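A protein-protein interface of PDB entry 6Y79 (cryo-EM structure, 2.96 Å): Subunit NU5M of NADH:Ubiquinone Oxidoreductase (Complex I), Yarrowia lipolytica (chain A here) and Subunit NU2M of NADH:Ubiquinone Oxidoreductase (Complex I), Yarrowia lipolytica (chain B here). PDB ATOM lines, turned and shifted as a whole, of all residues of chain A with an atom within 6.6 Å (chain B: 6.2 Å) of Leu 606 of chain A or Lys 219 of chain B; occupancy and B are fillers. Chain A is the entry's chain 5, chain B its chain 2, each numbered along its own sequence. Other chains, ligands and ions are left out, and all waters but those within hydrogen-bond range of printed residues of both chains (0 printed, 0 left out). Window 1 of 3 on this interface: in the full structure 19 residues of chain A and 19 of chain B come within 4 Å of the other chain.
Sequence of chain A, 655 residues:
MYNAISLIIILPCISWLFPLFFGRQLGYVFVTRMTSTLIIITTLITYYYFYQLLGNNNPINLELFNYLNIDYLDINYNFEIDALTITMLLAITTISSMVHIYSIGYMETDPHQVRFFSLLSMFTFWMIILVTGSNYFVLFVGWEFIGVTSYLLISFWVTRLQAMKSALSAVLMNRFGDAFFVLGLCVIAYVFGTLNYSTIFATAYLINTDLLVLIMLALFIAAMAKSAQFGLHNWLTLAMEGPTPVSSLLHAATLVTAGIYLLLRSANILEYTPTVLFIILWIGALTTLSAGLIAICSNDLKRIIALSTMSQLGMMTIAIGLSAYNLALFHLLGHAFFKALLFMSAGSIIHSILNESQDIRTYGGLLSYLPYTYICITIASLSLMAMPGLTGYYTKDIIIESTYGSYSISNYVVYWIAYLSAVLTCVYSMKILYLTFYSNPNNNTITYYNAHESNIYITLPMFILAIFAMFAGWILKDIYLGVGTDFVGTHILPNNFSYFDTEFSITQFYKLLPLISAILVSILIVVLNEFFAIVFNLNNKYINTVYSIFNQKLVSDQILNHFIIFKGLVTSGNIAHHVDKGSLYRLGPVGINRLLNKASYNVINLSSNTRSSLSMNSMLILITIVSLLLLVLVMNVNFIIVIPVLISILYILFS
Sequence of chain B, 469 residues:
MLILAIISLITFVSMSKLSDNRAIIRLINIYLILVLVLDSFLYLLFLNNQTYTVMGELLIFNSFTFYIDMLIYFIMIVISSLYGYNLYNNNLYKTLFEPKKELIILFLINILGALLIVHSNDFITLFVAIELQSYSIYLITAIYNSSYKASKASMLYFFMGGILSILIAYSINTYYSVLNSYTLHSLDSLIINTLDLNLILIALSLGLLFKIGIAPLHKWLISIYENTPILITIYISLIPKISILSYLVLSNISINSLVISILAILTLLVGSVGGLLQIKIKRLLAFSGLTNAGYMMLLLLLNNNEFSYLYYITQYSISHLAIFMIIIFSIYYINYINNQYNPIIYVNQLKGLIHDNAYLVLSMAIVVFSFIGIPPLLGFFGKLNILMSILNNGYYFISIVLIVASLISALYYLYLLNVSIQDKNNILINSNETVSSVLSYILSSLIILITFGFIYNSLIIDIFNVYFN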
ATOM      1  N   TYR A 601     -30.693   2.556   7.694  1.00  0.00           N
ATOM      2  CA  TYR A 601     -31.794   3.126   6.924  1.00  0.00           C
ATOM      3  C   TYR A 601     -31.784   4.646   6.994  1.00  0.00           C
ATOM      4  O   TYR A 601     -31.978   5.326   5.978  1.00  0.00           O
ATOM      5  CB  TYR A 601     -33.110   2.564   7.455  1.00  0.00           C
ATOM      6  CG  TYR A 601     -34.363   2.993   6.730  1.00  0.00           C
ATOM      7  CD1 TYR A 601     -34.682   2.468   5.489  1.00  0.00           C
ATOM      8  CD2 TYR A 601     -35.250   3.889   7.313  1.00  0.00           C
ATOM      9  CE1 TYR A 601     -35.838   2.840   4.833  1.00  0.00           C
ATOM     10  CE2 TYR A 601     -36.411   4.267   6.667  1.00  0.00           C
ATOM     11  CZ  TYR A 601     -36.699   3.738   5.427  1.00  0.00           C
ATOM     12  OH  TYR A 601     -37.851   4.112   4.770  1.00  0.00           O
ATOM     13  N   ASN A 602     -31.480   5.190   8.172  1.00  0.00           N
ATOM     14  CA  ASN A 602     -31.467   6.636   8.342  1.00  0.00           C
ATOM     15  C   ASN A 602     -30.291   7.277   7.613  1.00  0.00           C
ATOM     16  O   ASN A 602     -30.460   8.290   6.919  1.00  0.00           O
ATOM     17  CB  ASN A 602     -31.456   6.974   9.828  1.00  0.00           C
ATOM     18  CG  ASN A 602     -32.792   6.699  10.487  1.00  0.00           C
ATOM     19  OD1 ASN A 602     -32.869   6.044  11.520  1.00  0.00           O
ATOM     20  ND2 ASN A 602     -33.859   7.197   9.881  1.00  0.00           N
ATOM     21  N   VAL A 603     -29.097   6.689   7.713  1.00  0.00           N
ATOM     22  CA  VAL A 603     -27.969   7.302   7.013  1.00  0.00           C
ATOM     23  C   VAL A 603     -27.994   7.066   5.511  1.00  0.00           C
ATOM     24  O   VAL A 603     -27.293   7.767   4.778  1.00  0.00           O
ATOM     25  CB  VAL A 603     -26.611   6.837   7.552  1.00  0.00           C
ATOM     26  CG1 VAL A 603     -26.524   7.145   8.996  1.00  0.00           C
ATOM     27  CG2 VAL A 603     -26.410   5.372   7.312  1.00  0.00           C
ATOM     28  N   ILE A 604     -28.776   6.110   5.021  1.00  0.00           N
ATOM     29  CA  ILE A 604     -28.916   5.983   3.576  1.00  0.00           C
ATOM     30  C   ILE A 604     -29.967   6.956   3.058  1.00  0.00           C
ATOM     31  O   ILE A 604     -29.775   7.599   2.021  1.00  0.00           O
ATOM     32  CB  ILE A 604     -29.221   4.519   3.213  1.00  0.00           C
ATOM     33  CG1 ILE A 604     -27.964   3.682   3.380  1.00  0.00           C
ATOM     34  CG2 ILE A 604     -29.691   4.373   1.791  1.00  0.00           C
ATOM     35  CD1 ILE A 604     -28.242   2.222   3.426  1.00  0.00           C
ATOM     36  N   ASN A 605     -31.062   7.146   3.798  1.00  0.00           N
ATOM     37  CA  ASN A 605     -32.044   8.160   3.425  1.00  0.00           C
ATOM     38  C   ASN A 605     -31.616   9.580   3.769  1.00  0.00           C
ATOM     39  O   ASN A 605     -32.423  10.499   3.592  1.00  0.00           O
ATOM     40  CB  ASN A 605     -33.382   7.873   4.098  1.00  0.00           C
ATOM     41  CG  ASN A 605     -34.018   6.614   3.597  1.00  0.00           C
ATOM     42  OD1 ASN A 605     -34.077   6.364   2.397  1.00  0.00           O
ATOM     43  ND2 ASN A 605     -34.494   5.799   4.518  1.00  0.00           N
ATOM     44  N   LEU A 606     -30.405   9.759   4.305  1.00  0.00           N
ATOM     45  CA  LEU A 606     -29.835  11.091   4.501  1.00  0.00           C
ATOM     46  C   LEU A 606     -29.828  11.921   3.212  1.00  0.00           C
ATOM     47  O   LEU A 606     -30.076  13.130   3.250  1.00  0.00           O
ATOM     48  CB  LEU A 606     -28.425  10.946   5.084  1.00  0.00           C
ATOM     49  CG  LEU A 606     -27.593  12.141   5.553  1.00  0.00           C
ATOM     50  CD1 LEU A 606     -28.389  12.956   6.549  1.00  0.00           C
ATOM     51  CD2 LEU A 606     -26.287  11.663   6.197  1.00  0.00           C
ATOM     52  N   SER A 607     -29.579  11.303   2.061  1.00  0.00           N
ATOM     53  CA  SER A 607     -29.589  12.021   0.787  1.00  0.00           C
ATOM     54  C   SER A 607     -30.609  11.457  -0.198  1.00  0.00           C
ATOM     55  O   SER A 607     -30.328  11.302  -1.389  1.00  0.00           O
ATOM     56  CB  SER A 607     -28.209  12.014   0.154  1.00  0.00           C
ATOM     57  OG  SER A 607     -27.894  10.722  -0.327  1.00  0.00           O
ATOM     58  N   SER A 608     -31.802  11.141   0.289  1.00  0.00           N
ATOM     59  CA  SER A 608     -32.848  10.575  -0.548  1.00  0.00           C
ATOM     60  C   SER A 608     -33.670  11.648  -1.249  1.00  0.00           C
ATOM     61  O   SER A 608     -34.267  11.377  -2.299  1.00  0.00           O
ATOM     62  CB  SER A 608     -33.770   9.703   0.303  1.00  0.00           C
ATOM     63  OG  SER A 608     -34.357  10.471   1.344  1.00  0.00           O
ATOM     64  N   ASN A 609     -33.664  12.867  -0.691  1.00  0.00           N
ATOM     65  CA  ASN A 609     -34.703  13.868  -0.916  1.00  0.00           C
ATOM     66  C   ASN A 609     -34.763  14.348  -2.357  1.00  0.00           C
ATOM     67  O   ASN A 609     -35.741  14.097  -3.069  1.00  0.00           O
ATOM     68  CB  ASN A 609     -34.450  15.077  -0.012  1.00  0.00           C
ATOM     69  CG  ASN A 609     -35.010  14.899   1.376  1.00  0.00           C
ATOM     70  OD1 ASN A 609     -34.264  14.866   2.354  1.00  0.00           O
ATOM     71  ND2 ASN A 609     -36.330  14.807   1.477  1.00  0.00           N
ATOM     72  N   MET A 616     -28.023  19.056  -3.968  1.00  0.00           N
ATOM     73  CA  MET A 616     -27.953  18.266  -2.746  1.00  0.00           C
ATOM     74  C   MET A 616     -26.547  18.246  -2.168  1.00  0.00           C
ATOM     75  O   MET A 616     -26.334  18.639  -1.012  1.00  0.00           O
ATOM     76  CB  MET A 616     -28.431  16.852  -3.058  1.00  0.00           C
ATOM     77  CG  MET A 616     -28.185  15.821  -1.994  1.00  0.00           C
ATOM     78  SD  MET A 616     -28.349  14.184  -2.730  1.00  0.00           S
ATOM     79  CE  MET A 616     -30.103  14.156  -3.088  1.00  0.00           C
ATOM     80  N   ASN A 617     -25.562  17.844  -2.978  1.00  0.00           N
ATOM     81  CA  ASN A 617     -24.212  17.721  -2.442  1.00  0.00           C
ATOM     82  C   ASN A 617     -23.540  19.072  -2.213  1.00  0.00           C
ATOM     83  O   ASN A 617     -22.773  19.216  -1.257  1.00  0.00           O
ATOM     84  CB  ASN A 617     -23.379  16.845  -3.362  1.00  0.00           C
ATOM     85  CG  ASN A 617     -23.876  15.428  -3.393  1.00  0.00           C
ATOM     86  OD1 ASN A 617     -24.034  14.796  -2.353  1.00  0.00           O
ATOM     87  ND2 ASN A 617     -24.152  14.926  -4.581  1.00  0.00           N
ATOM     88  N   LEU A 620     -24.830  20.337   0.936  1.00  0.00           N
ATOM     89  CA  LEU A 620     -24.226  19.512   1.970  1.00  0.00           C
ATOM     90  C   LEU A 620     -22.808  19.953   2.309  1.00  0.00           C
ATOM     91  O   LEU A 620     -22.396  19.842   3.462  1.00  0.00           O
ATOM     92  CB  LEU A 620     -24.241  18.059   1.510  1.00  0.00           C
ATOM     93  CG  LEU A 620     -23.904  16.956   2.496  1.00  0.00           C
ATOM     94  CD1 LEU A 620     -24.774  17.113   3.703  1.00  0.00           C
ATOM     95  CD2 LEU A 620     -24.151  15.624   1.840  1.00  0.00           C
ATOM     96  N   ILE A 652     -29.848  12.949  15.209  1.00  0.00           N
ATOM     97  CA  ILE A 652     -30.573  13.310  13.998  1.00  0.00           C
ATOM     98  C   ILE A 652     -29.912  12.709  12.765  1.00  0.00           C
ATOM     99  O   ILE A 652     -30.542  12.613  11.709  1.00  0.00           O
ATOM    100  CB  ILE A 652     -30.726  14.834  13.874  1.00  0.00           C
ATOM    101  CG1 ILE A 652     -29.366  15.497  13.713  1.00  0.00           C
ATOM    102  CG2 ILE A 652     -31.457  15.390  15.079  1.00  0.00           C
ATOM    103  CD1 ILE A 652     -29.449  16.978  13.577  1.00  0.00           C
ATOM    104  N   LEU A 653     -28.655  12.276  12.870  1.00  0.00           N
ATOM    105  CA  LEU A 653     -27.982  11.666  11.729  1.00  0.00           C
ATOM    106  C   LEU A 653     -28.351  10.197  11.602  1.00  0.00           C
ATOM    107  O   LEU A 653     -28.624   9.708  10.501  1.00  0.00           O
ATOM    108  CB  LEU A 653     -26.469  11.836  11.876  1.00  0.00           C
ATOM    109  CG  LEU A 653     -25.489  11.619  10.724  1.00  0.00           C
ATOM    110  CD1 LEU A 653     -24.303  12.529  10.948  1.00  0.00           C
ATOM    111  CD2 LEU A 653     -25.006  10.175  10.583  1.00  0.00           C
ATOM    112  N   ALA B 215     -16.234  11.658   6.123  1.00  0.00           N
ATOM    113  CA  ALA B 215     -17.633  11.334   6.387  1.00  0.00           C
ATOM    114  C   ALA B 215     -18.768  12.328   6.181  1.00  0.00           C
ATOM    115  O   ALA B 215     -19.866  11.869   5.835  1.00  0.00           O
ATOM    116  CB  ALA B 215     -17.767  10.897   7.823  1.00  0.00           C
ATOM    117  N   PRO B 216     -18.639  13.633   6.470  1.00  0.00           N
ATOM    118  CA  PRO B 216     -19.784  14.506   6.191  1.00  0.00           C
ATOM    119  C   PRO B 216     -20.072  14.621   4.710  1.00  0.00           C
ATOM    120  O   PRO B 216     -21.231  14.796   4.319  1.00  0.00           O
ATOM    121  CB  PRO B 216     -19.353  15.842   6.799  1.00  0.00           C
ATOM    122  CG  PRO B 216     -18.339  15.515   7.769  1.00  0.00           C
ATOM    123  CD  PRO B 216     -17.590  14.400   7.171  1.00  0.00           C
ATOM    124  N   LEU B 217     -19.051  14.455   3.877  1.00  0.00           N
ATOM    125  CA  LEU B 217     -19.094  14.682   2.443  1.00  0.00           C
ATOM    126  C   LEU B 217     -18.663  13.435   1.705  1.00  0.00           C
ATOM    127  O   LEU B 217     -17.779  13.456   0.849  1.00  0.00           O
ATOM    128  CB  LEU B 217     -18.216  15.868   2.076  1.00  0.00           C
ATOM    129  CG  LEU B 217     -18.660  17.154   2.757  1.00  0.00           C
ATOM    130  CD1 LEU B 217     -17.777  18.310   2.365  1.00  0.00           C
ATOM    131  CD2 LEU B 217     -20.105  17.414   2.402  1.00  0.00           C
ATOM    132  N   HIS B 218     -19.275  12.312   2.050  1.00  0.00           N
ATOM    133  CA  HIS B 218     -18.869  11.032   1.503  1.00  0.00           C
ATOM    134  C   HIS B 218     -19.755  10.528   0.376  1.00  0.00           C
ATOM    135  O   HIS B 218     -19.286   9.724  -0.428  1.00  0.00           O
ATOM    136  CB  HIS B 218     -18.833   9.986   2.618  1.00  0.00           C
ATOM    137  CG  HIS B 218     -20.183   9.609   3.132  1.00  0.00           C
ATOM    138  ND1 HIS B 218     -20.893  10.398   4.010  1.00  0.00           N
ATOM    139  CD2 HIS B 218     -20.958   8.528   2.889  1.00  0.00           C
ATOM    140  CE1 HIS B 218     -22.048   9.820   4.282  1.00  0.00           C
ATOM    141  NE2 HIS B 218     -22.113   8.684   3.615  1.00  0.00           N
ATOM    142  N   LYS B 219     -20.996  11.003   0.267  1.00  0.00           N
ATOM    143  CA  LYS B 219     -21.986  10.337  -0.575  1.00  0.00           C
ATOM    144  C   LYS B 219     -21.750  10.581  -2.049  1.00  0.00           C
ATOM    145  O   LYS B 219     -22.073   9.728  -2.886  1.00  0.00           O
ATOM    146  CB  LYS B 219     -23.367  10.831  -0.218  1.00  0.00           C
ATOM    147  CG  LYS B 219     -23.723  10.526   1.168  1.00  0.00           C
ATOM    148  CD  LYS B 219     -24.985  11.203   1.471  1.00  0.00           C
ATOM    149  CE  LYS B 219     -25.610  10.607   2.709  1.00  0.00           C
ATOM    150  NZ  LYS B 219     -26.109   9.223   2.456  1.00  0.00           N
ATOM    151  N   TRP B 220     -21.255  11.767  -2.385  1.00  0.00           N
ATOM    152  CA  TRP B 220     -20.977  12.097  -3.772  1.00  0.00           C
ATOM    153  C   TRP B 220     -19.903  11.180  -4.347  1.00  0.00           C
ATOM    154  O   TRP B 220     -20.023  10.718  -5.484  1.00  0.00           O
ATOM    155  CB  TRP B 220     -20.588  13.570  -3.874  1.00  0.00           C
ATOM    156  CG  TRP B 220     -19.378  13.954  -3.119  1.00  0.00           C
ATOM    157  CD1 TRP B 220     -19.299  14.222  -1.798  1.00  0.00           C
ATOM    158  CD2 TRP B 220     -18.062  14.126  -3.644  1.00  0.00           C
ATOM    159  NE1 TRP B 220     -18.014  14.541  -1.455  1.00  0.00           N
ATOM    160  CE2 TRP B 220     -17.235  14.489  -2.578  1.00  0.00           C
ATOM    161  CE3 TRP B 220     -17.502  13.997  -4.915  1.00  0.00           C
ATOM    162  CZ2 TRP B 220     -15.881  14.729  -2.741  1.00  0.00           C
ATOM    163  CZ3 TRP B 220     -16.164  14.241  -5.075  1.00  0.00           C
ATOM    164  CH2 TRP B 220     -15.366  14.602  -3.998  1.00  0.00           C
ATOM    165  N   LEU B 221     -18.910  10.818  -3.536  1.00  0.00           N
ATOM    166  CA  LEU B 221     -17.869   9.915  -4.003  1.00  0.00           C
ATOM    167  C   LEU B 221     -18.363   8.479  -4.105  1.00  0.00           C
ATOM    168  O   LEU B 221     -17.935   7.746  -4.999  1.00  0.00           O
ATOM    169  CB  LEU B 221     -16.661   9.990  -3.088  1.00  0.00           C
ATOM    170  CG  LEU B 221     -15.597  10.939  -3.610  1.00  0.00           C
ATOM    171  CD1 LEU B 221     -14.565  11.142  -2.576  1.00  0.00           C
ATOM    172  CD2 LEU B 221     -14.966  10.417  -4.861  1.00  0.00           C
ATOM    173  N   ILE B 222     -19.251   8.052  -3.200  1.00  0.00           N
ATOM    174  CA  ILE B 222     -19.851   6.727  -3.320  1.00  0.00           C
ATOM    175  C   ILE B 222     -20.690   6.638  -4.588  1.00  0.00           C
ATOM    176  O   ILE B 222     -20.688   5.608  -5.276  1.00  0.00           O
ATOM    177  CB  ILE B 222     -20.691   6.382  -2.070  1.00  0.00           C
ATOM    178  CG1 ILE B 222     -19.907   6.578  -0.775  1.00  0.00           C
ATOM    179  CG2 ILE B 222     -21.155   4.952  -2.127  1.00  0.00           C
ATOM    180  CD1 ILE B 222     -18.740   5.670  -0.596  1.00  0.00           C
ATOM    181  N   SER B 223     -21.378   7.725  -4.948  1.00  0.00           N
ATOM    182  CA  SER B 223     -22.143   7.743  -6.191  1.00  0.00           C
ATOM    183  C   SER B 223     -21.237   7.732  -7.419  1.00  0.00           C
ATOM    184  O   SER B 223     -21.573   7.109  -8.430  1.00  0.00           O
ATOM    185  CB  SER B 223     -23.058   8.960  -6.222  1.00  0.00           C
ATOM    186  OG  SER B 223     -22.298  10.147  -6.276  1.00  0.00           O
ATOM    187  N   ILE B 224     -20.093   8.418  -7.358  1.00  0.00           N
ATOM    188  CA  ILE B 224     -19.146   8.372  -8.476  1.00  0.00           C
ATOM    189  C   ILE B 224     -18.558   6.973  -8.625  1.00  0.00           C
ATOM    190  O   ILE B 224     -18.399   6.466  -9.739  1.00  0.00           O
ATOM    191  CB  ILE B 224     -18.049   9.437  -8.298  1.00  0.00           C
ATOM    192  CG1 ILE B 224     -18.635  10.825  -8.443  1.00  0.00           C
ATOM    193  CG2 ILE B 224     -16.949   9.302  -9.326  1.00  0.00           C
ATOM    194  CD1 ILE B 224     -17.882  11.811  -7.696  1.00  0.00           C
ATOM    195  N   VAL B 270     -19.998   6.122  10.252  1.00  0.00           N
ATOM    196  CA  VAL B 270     -20.847   6.145   9.063  1.00  0.00           C
ATOM    197  C   VAL B 270     -20.365   5.204   7.972  1.00  0.00           C
ATOM    198  O   VAL B 270     -21.141   4.886   7.070  1.00  0.00           O
ATOM    199  CB  VAL B 270     -20.949   7.581   8.500  1.00  0.00           C
ATOM    200  CG1 VAL B 270     -19.785   7.909   7.626  1.00  0.00           C
ATOM    201  CG2 VAL B 270     -22.261   7.831   7.776  1.00  0.00           C
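The side-chain amino group (NZ) of Lys 219 of chain B lies within hydrogen-bond range of the backbone carbonyl oxygen (O) of Val 603 of chain A (3.0 Å).
NE1 of Trp 220 of chain B lies within hydrogen-bond range of O of Leu 217 of chain B, 2.6 Å away.
O of Lys 219 of chain B is in hydrogen-bond range of OG of Ser 223 of chain B (3.4 Å).
The backbone carbonyl oxygen (O) of Trp 220 of chain B sits at hydrogen-bond distance from the side-chain hydroxyl (OG) of Ser 223 of chain B (2.5 Å).
Leu 606 of chain A touches Lys 219 of chain B.
Ser 607 of chain A touches Lys 219 of chain B.
Asn 617 of chain A touches Trp 220 of chain B (CG to CB, 3.8 Å).
O of Pro 216 of chain B touches CG of Leu 620 of chain A, at 3.9 Å.
CD2 of Leu 217 of chain B touches O of Leu 620 of chain A, at 3.5 Å.
Of the printed residues of chain B, Leu 606 of chain A touches Lys 219.
Printed residues of chain B within 4 Å of Ser 607 of chain A: Lys 219.
Met 616 of chain A touches none of the printed residues of chain B.
Printed residues of chain B within 4 Å of Asn 617 of chain A: Trp 220 (3.8 Å).
Of the printed residues of chain B, Leu 620 of chain A touches Pro 216 (3.9 Å) and Leu 217 (3.5 Å).
Printed residues of chain A within 4 Å of Pro 216 of chain B: Leu 620 (3.9 Å).
Lys 219 of chain B touches three residues of chain A.
Printed residues of chain A within 4 Å of Trp 220 of chain B: Asn 617 (3.8 Å).
The nearest residue of chain A that does not touch Lys 219 of chain B is Ile 604 of chain A (4.03 Å).
Of the 11 printed residues of chain B, 4 touch a printed residue of chain A.
Printed residues of chain B that touch a printed residue of chain A: Pro 216, Leu 217, Lys 219 and Trp 220.
Along chain B the printed residues that touch a printed residue of chain A span positions 216 to 220.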
